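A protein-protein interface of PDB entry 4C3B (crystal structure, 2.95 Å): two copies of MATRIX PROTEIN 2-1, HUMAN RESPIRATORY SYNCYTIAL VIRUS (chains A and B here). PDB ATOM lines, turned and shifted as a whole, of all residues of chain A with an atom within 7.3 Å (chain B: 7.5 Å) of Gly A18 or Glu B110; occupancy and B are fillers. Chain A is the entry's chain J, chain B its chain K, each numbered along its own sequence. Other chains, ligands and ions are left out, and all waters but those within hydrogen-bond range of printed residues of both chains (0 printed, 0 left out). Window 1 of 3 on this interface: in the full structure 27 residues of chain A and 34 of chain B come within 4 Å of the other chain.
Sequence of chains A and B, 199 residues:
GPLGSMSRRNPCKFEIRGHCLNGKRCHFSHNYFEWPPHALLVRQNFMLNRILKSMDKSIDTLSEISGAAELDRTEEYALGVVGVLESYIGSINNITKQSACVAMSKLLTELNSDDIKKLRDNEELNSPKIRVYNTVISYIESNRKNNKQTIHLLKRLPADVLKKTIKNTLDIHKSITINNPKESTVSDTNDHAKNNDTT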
ATOM      1  N   CYS A  12      23.355  31.207 -11.045  1.00  0.00           N
ATOM      2  CA  CYS A  12      24.689  30.736 -11.336  1.00  0.00           C
ATOM      3  C   CYS A  12      25.267  31.359 -12.599  1.00  0.00           C
ATOM      4  O   CYS A  12      24.752  31.152 -13.694  1.00  0.00           O
ATOM      5  CB  CYS A  12      24.664  29.242 -11.537  1.00  0.00           C
ATOM      6  SG  CYS A  12      26.238  28.511 -12.043  1.00  0.00           S
ATOM      7  N   LYS A  13      26.342  32.130 -12.445  1.00  0.00           N
ATOM      8  CA  LYS A  13      26.965  32.823 -13.563  1.00  0.00           C
ATOM      9  C   LYS A  13      27.555  31.849 -14.563  1.00  0.00           C
ATOM     10  O   LYS A  13      27.717  32.190 -15.702  1.00  0.00           O
ATOM     11  CB  LYS A  13      28.010  33.829 -13.073  1.00  0.00           C
ATOM     12  CG  LYS A  13      27.385  35.067 -12.411  1.00  0.00           C
ATOM     13  CD  LYS A  13      28.383  35.992 -11.698  1.00  0.00           C
ATOM     14  CE  LYS A  13      29.383  36.692 -12.645  1.00  0.00           C
ATOM     15  NZ  LYS A  13      28.800  37.451 -13.802  1.00  0.00           N
ATOM     16  N   PHE A  14      27.878  30.637 -14.163  1.00  0.00           N
ATOM     17  CA  PHE A  14      28.358  29.665 -15.137  1.00  0.00           C
ATOM     18  C   PHE A  14      27.225  29.262 -16.059  1.00  0.00           C
ATOM     19  O   PHE A  14      27.473  29.048 -17.240  1.00  0.00           O
ATOM     20  CB  PHE A  14      28.917  28.392 -14.456  1.00  0.00           C
ATOM     21  CG  PHE A  14      30.250  28.588 -13.833  1.00  0.00           C
ATOM     22  CD1 PHE A  14      30.341  29.118 -12.536  1.00  0.00           C
ATOM     23  CD2 PHE A  14      31.401  28.292 -14.537  1.00  0.00           C
ATOM     24  CE1 PHE A  14      31.566  29.342 -11.970  1.00  0.00           C
ATOM     25  CE2 PHE A  14      32.627  28.501 -13.971  1.00  0.00           C
ATOM     26  CZ  PHE A  14      32.710  29.020 -12.683  1.00  0.00           C
ATOM     27  N   GLU A  15      26.026  29.088 -15.472  1.00  0.00           N
ATOM     28  CA  GLU A  15      24.805  28.666 -16.159  1.00  0.00           C
ATOM     29  C   GLU A  15      24.348  29.789 -17.043  1.00  0.00           C
ATOM     30  O   GLU A  15      23.855  29.548 -18.137  1.00  0.00           O
ATOM     31  CB  GLU A  15      23.656  28.356 -15.165  1.00  0.00           C
ATOM     32  CG  GLU A  15      22.368  27.769 -15.761  1.00  0.00           C
ATOM     33  CD  GLU A  15      22.539  26.341 -16.265  1.00  0.00           C
ATOM     34  OE1 GLU A  15      23.527  25.671 -15.895  1.00  0.00           O
ATOM     35  OE2 GLU A  15      21.720  25.880 -17.079  1.00  0.00           O
ATOM     36  N   ILE A  16      24.488  31.015 -16.563  1.00  0.00           N
ATOM     37  CA  ILE A  16      24.215  32.134 -17.415  1.00  0.00           C
ATOM     38  C   ILE A  16      24.960  32.007 -18.757  1.00  0.00           C
ATOM     39  O   ILE A  16      24.455  32.404 -19.757  1.00  0.00           O
ATOM     40  CB  ILE A  16      24.500  33.473 -16.747  1.00  0.00           C
ATOM     41  CG1 ILE A  16      23.537  33.653 -15.593  1.00  0.00           C
ATOM     42  CG2 ILE A  16      24.270  34.582 -17.737  1.00  0.00           C
ATOM     43  CD1 ILE A  16      23.469  35.079 -15.018  1.00  0.00           C
ATOM     44  N   ARG A  17      26.146  31.455 -18.799  1.00  0.00           N
ATOM     45  CA  ARG A  17      26.858  31.404 -20.059  1.00  0.00           C
ATOM     46  C   ARG A  17      26.636  30.090 -20.769  1.00  0.00           C
ATOM     47  O   ARG A  17      27.308  29.774 -21.779  1.00  0.00           O
ATOM     48  CB  ARG A  17      28.362  31.595 -19.807  1.00  0.00           C
ATOM     49  CG  ARG A  17      28.683  32.841 -19.021  1.00  0.00           C
ATOM     50  CD  ARG A  17      30.153  32.907 -18.619  1.00  0.00           C
ATOM     51  NE  ARG A  17      30.578  34.288 -18.830  1.00  0.00           N
ATOM     52  CZ  ARG A  17      31.142  34.717 -19.939  1.00  0.00           C
ATOM     53  NH1 ARG A  17      31.436  33.890 -20.970  1.00  0.00           N
ATOM     54  NH2 ARG A  17      31.433  35.988 -20.001  1.00  0.00           N
ATOM     55  N   GLY A  18      25.824  29.249 -20.166  1.00  0.00           N
ATOM     56  CA  GLY A  18      25.623  27.943 -20.738  1.00  0.00           C
ATOM     57  C   GLY A  18      25.254  26.930 -19.709  1.00  0.00           C
ATOM     58  O   GLY A  18      24.181  26.992 -19.180  1.00  0.00           O
ATOM     59  N   HIS A  19      26.155  25.996 -19.438  1.00  0.00           N
ATOM     60  CA  HIS A  19      25.890  24.922 -18.508  1.00  0.00           C
ATOM     61  C   HIS A  19      26.887  24.904 -17.365  1.00  0.00           C
ATOM     62  O   HIS A  19      28.043  24.596 -17.578  1.00  0.00           O
ATOM     63  CB  HIS A  19      25.872  23.609 -19.268  1.00  0.00           C
ATOM     64  CG  HIS A  19      24.791  23.563 -20.314  1.00  0.00           C
ATOM     65  ND1 HIS A  19      23.439  23.568 -19.996  1.00  0.00           N
ATOM     66  CD2 HIS A  19      24.858  23.526 -21.667  1.00  0.00           C
ATOM     67  CE1 HIS A  19      22.729  23.520 -21.110  1.00  0.00           C
ATOM     68  NE2 HIS A  19      23.564  23.490 -22.136  1.00  0.00           N
ATOM     69  N   CYS A  20      26.445  25.304 -16.170  1.00  0.00           N
ATOM     70  CA  CYS A  20      27.246  25.138 -14.934  1.00  0.00           C
ATOM     71  C   CYS A  20      27.845  23.721 -14.801  1.00  0.00           C
ATOM     72  O   CYS A  20      27.160  22.788 -15.038  1.00  0.00           O
ATOM     73  CB  CYS A  20      26.413  25.472 -13.705  1.00  0.00           C
ATOM     74  SG  CYS A  20      27.289  25.174 -12.173  1.00  0.00           S
ATOM     75  N   LEU A  21      29.132  23.579 -14.489  1.00  0.00           N
ATOM     76  CA  LEU A  21      29.767  22.261 -14.566  1.00  0.00           C
ATOM     77  C   LEU A  21      30.240  21.797 -13.197  1.00  0.00           C
ATOM     78  O   LEU A  21      31.027  20.837 -13.089  1.00  0.00           O
ATOM     79  CB  LEU A  21      30.957  22.279 -15.543  1.00  0.00           C
ATOM     80  CG  LEU A  21      30.669  22.481 -17.018  1.00  0.00           C
ATOM     81  CD1 LEU A  21      31.917  22.377 -17.866  1.00  0.00           C
ATOM     82  CD2 LEU A  21      29.671  21.431 -17.454  1.00  0.00           C
ATOM     83  N   TYR A  32      15.608  28.107 -13.820  1.00  0.00           N
ATOM     84  CA  TYR A  32      15.233  29.297 -14.567  1.00  0.00           C
ATOM     85  C   TYR A  32      14.018  29.994 -13.977  1.00  0.00           C
ATOM     86  O   TYR A  32      13.930  31.234 -14.036  1.00  0.00           O
ATOM     87  CB  TYR A  32      15.025  28.988 -16.034  1.00  0.00           C
ATOM     88  CG  TYR A  32      16.193  28.287 -16.656  1.00  0.00           C
ATOM     89  CD1 TYR A  32      17.473  28.704 -16.419  1.00  0.00           C
ATOM     90  CD2 TYR A  32      16.021  27.176 -17.458  1.00  0.00           C
ATOM     91  CE1 TYR A  32      18.560  28.034 -16.970  1.00  0.00           C
ATOM     92  CE2 TYR A  32      17.096  26.508 -18.022  1.00  0.00           C
ATOM     93  CZ  TYR A  32      18.356  26.950 -17.782  1.00  0.00           C
ATOM     94  OH  TYR A  32      19.431  26.366 -18.380  1.00  0.00           O
ATOM     95  N   TRP A  35      15.024  32.764 -11.572  1.00  0.00           N
ATOM     96  CA  TRP A  35      15.937  33.812 -12.069  1.00  0.00           C
ATOM     97  C   TRP A  35      15.172  35.073 -12.372  1.00  0.00           C
ATOM     98  O   TRP A  35      14.047  35.022 -12.823  1.00  0.00           O
ATOM     99  CB  TRP A  35      16.610  33.384 -13.357  1.00  0.00           C
ATOM    100  CG  TRP A  35      17.662  32.370 -13.173  1.00  0.00           C
ATOM    101  CD1 TRP A  35      17.802  31.527 -12.135  1.00  0.00           C
ATOM    102  CD2 TRP A  35      18.677  32.027 -14.116  1.00  0.00           C
ATOM    103  NE1 TRP A  35      18.853  30.679 -12.356  1.00  0.00           N
ATOM    104  CE2 TRP A  35      19.400  30.958 -13.574  1.00  0.00           C
ATOM    105  CE3 TRP A  35      19.029  32.519 -15.364  1.00  0.00           C
ATOM    106  CZ2 TRP A  35      20.466  30.387 -14.215  1.00  0.00           C
ATOM    107  CZ3 TRP A  35      20.079  31.965 -15.997  1.00  0.00           C
ATOM    108  CH2 TRP A  35      20.806  30.908 -15.420  1.00  0.00           C
ATOM    109  N   ARG A  43      21.508  34.947 -20.780  1.00  0.00           N
ATOM    110  CA  ARG A  43      21.785  33.567 -21.064  1.00  0.00           C
ATOM    111  C   ARG A  43      21.364  33.215 -22.480  1.00  0.00           C
ATOM    112  O   ARG A  43      22.094  32.514 -23.194  1.00  0.00           O
ATOM    113  CB  ARG A  43      21.116  32.631 -20.055  1.00  0.00           C
ATOM    114  CG  ARG A  43      21.397  31.165 -20.316  1.00  0.00           C
ATOM    115  CD  ARG A  43      20.858  30.230 -19.236  1.00  0.00           C
ATOM    116  NE  ARG A  43      21.455  28.920 -19.526  1.00  0.00           N
ATOM    117  CZ  ARG A  43      20.972  28.027 -20.387  1.00  0.00           C
ATOM    118  NH1 ARG A  43      19.792  28.193 -20.988  1.00  0.00           N
ATOM    119  NH2 ARG A  43      21.645  26.925 -20.602  1.00  0.00           N
ATOM    120  N   PHE A  46      24.117  34.201 -24.896  1.00  0.00           N
ATOM    121  CA  PHE A  46      25.273  33.315 -24.935  1.00  0.00           C
ATOM    122  C   PHE A  46      24.936  32.002 -25.617  1.00  0.00           C
ATOM    123  O   PHE A  46      25.768  31.424 -26.336  1.00  0.00           O
ATOM    124  CB  PHE A  46      25.806  33.030 -23.543  1.00  0.00           C
ATOM    125  CG  PHE A  46      26.583  34.165 -22.948  1.00  0.00           C
ATOM    126  CD1 PHE A  46      27.856  34.450 -23.379  1.00  0.00           C
ATOM    127  CD2 PHE A  46      26.026  34.965 -21.921  1.00  0.00           C
ATOM    128  CE1 PHE A  46      28.543  35.516 -22.844  1.00  0.00           C
ATOM    129  CE2 PHE A  46      26.729  36.022 -21.370  1.00  0.00           C
ATOM    130  CZ  PHE A  46      27.978  36.309 -21.848  1.00  0.00           C
ATOM    131  N   MET A  47      23.726  31.512 -25.379  1.00  0.00           N
ATOM    132  CA  MET A  47      23.325  30.215 -25.917  1.00  0.00           C
ATOM    133  C   MET A  47      23.083  30.313 -27.431  1.00  0.00           C
ATOM    134  O   MET A  47      23.563  29.465 -28.211  1.00  0.00           O
ATOM    135  CB  MET A  47      22.066  29.724 -25.196  1.00  0.00           C
ATOM    136  CG  MET A  47      22.280  29.156 -23.788  1.00  0.00           C
ATOM    137  SD  MET A  47      23.160  27.573 -23.915  1.00  0.00           S
ATOM    138  CE  MET A  47      21.942  26.481 -24.607  1.00  0.00           C
ATOM    139  N   ARG A  50      26.355  30.178 -29.146  1.00  0.00           N
ATOM    140  CA  ARG A  50      26.891  28.829 -29.167  1.00  0.00           C
ATOM    141  C   ARG A  50      26.247  28.005 -30.223  1.00  0.00           C
ATOM    142  O   ARG A  50      26.922  27.220 -30.884  1.00  0.00           O
ATOM    143  CB  ARG A  50      26.705  28.141 -27.811  1.00  0.00           C
ATOM    144  CG  ARG A  50      27.765  28.623 -26.833  1.00  0.00           C
ATOM    145  CD  ARG A  50      27.747  27.951 -25.478  1.00  0.00           C
ATOM    146  NE  ARG A  50      27.952  26.523 -25.581  1.00  0.00           N
ATOM    147  CZ  ARG A  50      27.982  25.731 -24.523  1.00  0.00           C
ATOM    148  NH1 ARG A  50      27.842  26.275 -23.305  1.00  0.00           N
ATOM    149  NH2 ARG A  50      28.159  24.412 -24.676  1.00  0.00           N
ATOM    150  N   ASN B  45      14.763  29.552 -22.593  1.00  0.00           N
ATOM    151  CA  ASN B  45      15.894  28.853 -22.040  1.00  0.00           C
ATOM    152  C   ASN B  45      15.807  27.328 -22.126  1.00  0.00           C
ATOM    153  O   ASN B  45      16.778  26.674 -22.505  1.00  0.00           O
ATOM    154  CB  ASN B  45      16.144  29.353 -20.654  1.00  0.00           C
ATOM    155  CG  ASN B  45      16.942  30.632 -20.665  1.00  0.00           C
ATOM    156  OD1 ASN B  45      18.150  30.577 -20.895  1.00  0.00           O
ATOM    157  ND2 ASN B  45      16.283  31.784 -20.450  1.00  0.00           N
ATOM    158  N   ASN B  49      18.193  25.031 -24.674  1.00  0.00           N
ATOM    159  CA  ASN B  49      18.933  23.859 -24.181  1.00  0.00           C
ATOM    160  C   ASN B  49      18.688  22.637 -25.048  1.00  0.00           C
ATOM    161  O   ASN B  49      19.605  21.870 -25.329  1.00  0.00           O
ATOM    162  CB  ASN B  49      18.586  23.587 -22.726  1.00  0.00           C
ATOM    163  CG  ASN B  49      19.113  24.661 -21.796  1.00  0.00           C
ATOM    164  OD1 ASN B  49      19.859  25.529 -22.209  1.00  0.00           O
ATOM    165  ND2 ASN B  49      18.721  24.604 -20.538  1.00  0.00           N
ATOM    166  N   LEU B  52      20.298  22.936 -28.519  1.00  0.00           N
ATOM    167  CA  LEU B  52      21.723  22.722 -28.460  1.00  0.00           C
ATOM    168  C   LEU B  52      22.023  21.257 -28.288  1.00  0.00           C
ATOM    169  O   LEU B  52      22.890  20.726 -28.992  1.00  0.00           O
ATOM    170  CB  LEU B  52      22.324  23.544 -27.344  1.00  0.00           C
ATOM    171  CG  LEU B  52      23.830  23.450 -27.173  1.00  0.00           C
ATOM    172  CD1 LEU B  52      24.573  23.592 -28.502  1.00  0.00           C
ATOM    173  CD2 LEU B  52      24.235  24.548 -26.191  1.00  0.00           C
ATOM    174  N   MET B 104      37.490  16.570 -19.873  1.00  0.00           N
ATOM    175  CA  MET B 104      38.235  17.683 -20.477  1.00  0.00           C
ATOM    176  C   MET B 104      37.532  18.132 -21.759  1.00  0.00           C
ATOM    177  O   MET B 104      37.286  19.316 -21.961  1.00  0.00           O
ATOM    178  CB  MET B 104      39.680  17.268 -20.785  1.00  0.00           C
ATOM    179  CG  MET B 104      40.575  18.393 -21.258  1.00  0.00           C
ATOM    180  SD  MET B 104      40.552  19.757 -20.095  1.00  0.00           S
ATOM    181  CE  MET B 104      41.696  20.867 -20.934  1.00  0.00           C
ATOM    182  N   SER B 105      37.184  17.165 -22.600  1.00  0.00           N
ATOM    183  CA  SER B 105      36.428  17.474 -23.788  1.00  0.00           C
ATOM    184  C   SER B 105      35.135  18.266 -23.460  1.00  0.00           C
ATOM    185  O   SER B 105      34.829  19.263 -24.087  1.00  0.00           O
ATOM    186  CB  SER B 105      36.121  16.194 -24.562  1.00  0.00           C
ATOM    187  OG  SER B 105      35.416  16.512 -25.743  1.00  0.00           O
ATOM    188  N   LYS B 106      34.382  17.826 -22.473  1.00  0.00           N
ATOM    189  CA  LYS B 106      33.137  18.505 -22.136  1.00  0.00           C
ATOM    190  C   LYS B 106      33.411  19.944 -21.697  1.00  0.00           C
ATOM    191  O   LYS B 106      32.620  20.834 -21.926  1.00  0.00           O
ATOM    192  CB  LYS B 106      32.359  17.741 -21.044  1.00  0.00           C
ATOM    193  CG  LYS B 106      32.209  16.217 -21.197  1.00  0.00           C
ATOM    194  CD  LYS B 106      31.018  15.765 -22.055  1.00  0.00           C
ATOM    195  CE  LYS B 106      29.725  15.546 -21.264  1.00  0.00           C
ATOM    196  NZ  LYS B 106      29.841  14.393 -20.333  1.00  0.00           N
ATOM    197  N   LEU B 107      34.547  20.178 -21.042  1.00  0.00           N
ATOM    198  CA  LEU B 107      34.883  21.521 -20.560  1.00  0.00           C
ATOM    199  C   LEU B 107      35.242  22.423 -21.734  1.00  0.00           C
ATOM    200  O   LEU B 107      34.802  23.577 -21.817  1.00  0.00           O
ATOM    201  CB  LEU B 107      36.049  21.450 -19.594  1.00  0.00           C
ATOM    202  CG  LEU B 107      36.541  22.802 -19.075  1.00  0.00           C
ATOM    203  CD1 LEU B 107      35.503  23.587 -18.270  1.00  0.00           C
ATOM    204  CD2 LEU B 107      37.796  22.561 -18.252  1.00  0.00           C
ATOM    205  N   LEU B 108      36.028  21.878 -22.659  1.00  0.00           N
ATOM    206  CA  LEU B 108      36.451  22.617 -23.847  1.00  0.00           C
ATOM    207  C   LEU B 108      35.249  23.060 -24.664  1.00  0.00           C
ATOM    208  O   LEU B 108      35.129  24.213 -25.059  1.00  0.00           O
ATOM    209  CB  LEU B 108      37.356  21.735 -24.696  1.00  0.00           C
ATOM    210  CG  LEU B 108      38.726  21.397 -24.088  1.00  0.00           C
ATOM    211  CD1 LEU B 108      39.463  20.388 -24.950  1.00  0.00           C
ATOM    212  CD2 LEU B 108      39.548  22.668 -23.907  1.00  0.00           C
ATOM    213  N   THR B 109      34.324  22.135 -24.855  1.00  0.00           N
ATOM    214  CA  THR B 109      33.045  22.457 -25.445  1.00  0.00           C
ATOM    215  C   THR B 109      32.329  23.630 -24.778  1.00  0.00           C
ATOM    216  O   THR B 109      31.706  24.421 -25.439  1.00  0.00           O
ATOM    217  CB  THR B 109      32.118  21.244 -25.413  1.00  0.00           C
ATOM    218  OG1 THR B 109      32.714  20.208 -26.195  1.00  0.00           O
ATOM    219  CG2 THR B 109      30.765  21.592 -25.988  1.00  0.00           C
ATOM    220  N   GLU B 110      32.382  23.721 -23.478  1.00  0.00           N
ATOM    221  CA  GLU B 110      31.655  24.757 -22.800  1.00  0.00           C
ATOM    222  C   GLU B 110      32.351  26.084 -22.970  1.00  0.00           C
ATOM    223  O   GLU B 110      31.769  27.129 -22.714  1.00  0.00           O
ATOM    224  CB  GLU B 110      31.553  24.402 -21.327  1.00  0.00           C
ATOM    225  CG  GLU B 110      30.838  25.432 -20.471  1.00  0.00           C
ATOM    226  CD  GLU B 110      29.375  25.491 -20.750  1.00  0.00           C
ATOM    227  OE1 GLU B 110      28.819  24.468 -21.283  1.00  0.00           O
ATOM    228  OE2 GLU B 110      28.797  26.544 -20.396  1.00  0.00           O
ATOM    229  N   LEU B 111      33.617  26.055 -23.372  1.00  0.00           N
ATOM    230  CA  LEU B 111      34.373  27.295 -23.543  1.00  0.00           C
ATOM    231  C   LEU B 111      34.277  27.779 -24.970  1.00  0.00           C
ATOM    232  O   LEU B 111      34.151  26.977 -25.898  1.00  0.00           O
ATOM    233  CB  LEU B 111      35.856  27.067 -23.214  1.00  0.00           C
ATOM    234  CG  LEU B 111      36.210  26.965 -21.741  1.00  0.00           C
ATOM    235  CD1 LEU B 111      37.699  26.683 -21.642  1.00  0.00           C
ATOM    236  CD2 LEU B 111      35.834  28.234 -20.986  1.00  0.00           C
ATOM    237  N   ASN B 112      34.425  29.083 -25.157  1.00  0.00           N
ATOM    238  CA  ASN B 112      34.555  29.577 -26.510  1.00  0.00           C
ATOM    239  C   ASN B 112      35.822  30.414 -26.797  1.00  0.00           C
ATOM    240  O   ASN B 112      36.128  31.407 -26.123  1.00  0.00           O
ATOM    241  CB  ASN B 112      33.258  30.271 -26.945  1.00  0.00           C
ATOM    242  CG  ASN B 112      33.202  31.719 -26.535  1.00  0.00           C
ATOM    243  OD1 ASN B 112      33.393  32.060 -25.370  1.00  0.00           O
ATOM    244  ND2 ASN B 112      32.946  32.585 -27.502  1.00  0.00           N
ATOM    245  N   ASP B 115      36.272  34.235 -26.172  1.00  0.00           N
ATOM    246  CA  ASP B 115      36.498  34.758 -24.836  1.00  0.00           C
ATOM    247  C   ASP B 115      37.989  34.688 -24.421  1.00  0.00           C
ATOM    248  O   ASP B 115      38.492  35.610 -23.757  1.00  0.00           O
ATOM    249  CB  ASP B 115      35.607  34.037 -23.831  1.00  0.00           C
ATOM    250  CG  ASP B 115      34.200  34.547 -23.850  1.00  0.00           C
ATOM    251  OD1 ASP B 115      34.015  35.730 -24.167  1.00  0.00           O
ATOM    252  OD2 ASP B 115      33.284  33.802 -23.468  1.00  0.00           O
ATOM    253  N   ILE B 140      40.507  23.764 -27.751  1.00  0.00           N
ATOM    254  CA  ILE B 140      39.114  24.077 -28.062  1.00  0.00           C
ATOM    255  C   ILE B 140      38.772  23.807 -29.537  1.00  0.00           C
ATOM    256  O   ILE B 140      37.713  23.257 -29.828  1.00  0.00           O
ATOM    257  CB  ILE B 140      38.783  25.531 -27.742  1.00  0.00           C
ATOM    258  CG1 ILE B 140      38.776  25.725 -26.224  1.00  0.00           C
ATOM    259  CG2 ILE B 140      37.439  25.919 -28.348  1.00  0.00           C
ATOM    260  CD1 ILE B 140      38.500  27.142 -25.743  1.00  0.00           C
ATOM    261  N   ASN B 143      38.821  20.204 -30.572  1.00  0.00           N
ATOM    262  CA  ASN B 143      37.655  19.607 -29.913  1.00  0.00           C
ATOM    263  C   ASN B 143      36.381  19.826 -30.712  1.00  0.00           C
ATOM    264  O   ASN B 143      35.618  18.883 -30.900  1.00  0.00           O
ATOM    265  CB  ASN B 143      37.488  20.206 -28.514  1.00  0.00           C
ATOM    266  CG  ASN B 143      36.610  19.367 -27.608  1.00  0.00           C
ATOM    267  OD1 ASN B 143      36.846  18.168 -27.441  1.00  0.00           O
ATOM    268  ND2 ASN B 143      35.598  20.005 -26.991  1.00  0.00           N
ATOM    269  N   HIS B 173      38.390  29.008 -17.428  1.00  0.00           N
ATOM    270  CA  HIS B 173      36.969  28.759 -17.211  1.00  0.00           C
ATOM    271  C   HIS B 173      36.441  29.538 -16.011  1.00  0.00           C
ATOM    272  O   HIS B 173      35.438  30.230 -16.138  1.00  0.00           O
ATOM    273  CB  HIS B 173      36.753  27.258 -17.046  1.00  0.00           C
ATOM    274  CG  HIS B 173      35.337  26.850 -16.775  1.00  0.00           C
ATOM    275  ND1 HIS B 173      34.296  27.156 -17.617  1.00  0.00           N
ATOM    276  CD2 HIS B 173      34.803  26.108 -15.773  1.00  0.00           C
ATOM    277  CE1 HIS B 173      33.175  26.654 -17.129  1.00  0.00           C
ATOM    278  NE2 HIS B 173      33.456  26.008 -16.015  1.00  0.00           N
ATOM    279  N   ILE B 176      37.024  33.684 -16.823  1.00  0.00           N
ATOM    280  CA  ILE B 176      36.017  34.207 -17.735  1.00  0.00           C
ATOM    281  C   ILE B 176      34.690  34.445 -17.021  1.00  0.00           C
ATOM    282  O   ILE B 176      34.085  35.494 -17.160  1.00  0.00           O
ATOM    283  CB  ILE B 176      35.760  33.216 -18.860  1.00  0.00           C
ATOM    284  CG1 ILE B 176      36.939  33.178 -19.802  1.00  0.00           C
ATOM    285  CG2 ILE B 176      34.525  33.602 -19.643  1.00  0.00           C
ATOM    286  CD1 ILE B 176      36.893  32.035 -20.807  1.00  0.00           C
ATOM    287  N   THR B 177      34.223  33.445 -16.285  1.00  0.00           N
ATOM    288  CA  THR B 177      32.903  33.464 -15.702  1.00  0.00           C
ATOM    289  C   THR B 177      32.746  34.505 -14.615  1.00  0.00           C
ATOM    290  O   THR B 177      31.644  34.966 -14.353  1.00  0.00           O
ATOM    291  CB  THR B 177      32.557  32.068 -15.197  1.00  0.00           C
ATOM    292  OG1 THR B 177      32.525  31.143 -16.305  1.00  0.00           O
ATOM    293  CG2 THR B 177      31.232  32.062 -14.501  1.00  0.00           C
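NH1 of Arg A17 lies within salt-bridge range of OD2 of Asp B115 (3.1 Å).
N of His A19 sits at hydrogen-bond distance from OE2 of Glu B110, 2.9 Å away.
The side-chain hydroxyl of Tyr A32 is in hydrogen-bond range of the side-chain amide nitrogen of Asn B49.
NH1 of Arg A43 is in hydrogen-bond range of OD1 of Asn B45, at 2.9 Å.
The guanidinium group (NH2) of Arg A43 sits at hydrogen-bond distance from the side-chain amide oxygen (OD1) of Asn B49, 2.8 Å away.
The guanidinium group of Arg A50 is in salt-bridge range of the side-chain carboxylate of Glu B110, at 2.9 Å.
OE2 of Glu A15 sits at hydrogen-bond distance from OH of Tyr A32, at 2.7 Å.
The guanidinium group (NH2) of Arg A43 sits at hydrogen-bond distance from the side-chain sulfur (SD) of Met A47, 3.7 Å away.
The backbone carbonyl oxygen (O) of Asn B45 sits close to the side-chain amide oxygen (OD1) of Asn B49 (3.3 Å).
O of Ser B105 lies within hydrogen-bond range of OG1 of Thr B109 (3.1 Å).
OG1 of Thr B109 lies within hydrogen-bond range of ND2 of Asn B143 (3.0 Å).
The side-chain amide oxygen (OD1) of Asn B112 sits close to the side-chain carboxylate (OD2) of Asp B115 (2.6 Å).
Among the printed residues, pairs that only touch across the chains: Met A47 with Asn B49, Lys A13 with Thr B177, Phe A14 with His B173, Arg A17 with Ile B176, Met A47 with Leu B52, Gly A18 with Glu B110, Phe A14 with Thr B177, Arg A50 with Thr B109, His A19 with Asn B49, Arg A17 with Thr B177, Leu A21 with Leu B107, Arg A17 with Glu B110 and Tyr A32 with Asn B45.
Of the printed residues of chain B, Phe A14 touches His B173 (3.3 Å) and Thr B177 (3.5 Å).
Gly A18 touches just one residue of chain B: Glu B110.
Of the printed residues of chain B, His A19 touches Asn B49 (3.7 Å) and Glu B110 (2.9 Å).
Of the printed residues of chain B, Tyr A32 touches Asn B45 and Asn B49.
Glu B110 touches four residues of chain A.
Printed residues of chain A within 4 Å of Asp B115: Arg A17.
The nearest residue of chain A that does not touch Glu B110 is Leu A21 (4.03 Å).
The nearest printed residue of chain B that does not touch His A19 is Leu B52 (4.2 Å).
Of the 16 printed residues of chain A, 10 touch a printed residue of chain B.
No position is printed for both chains.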
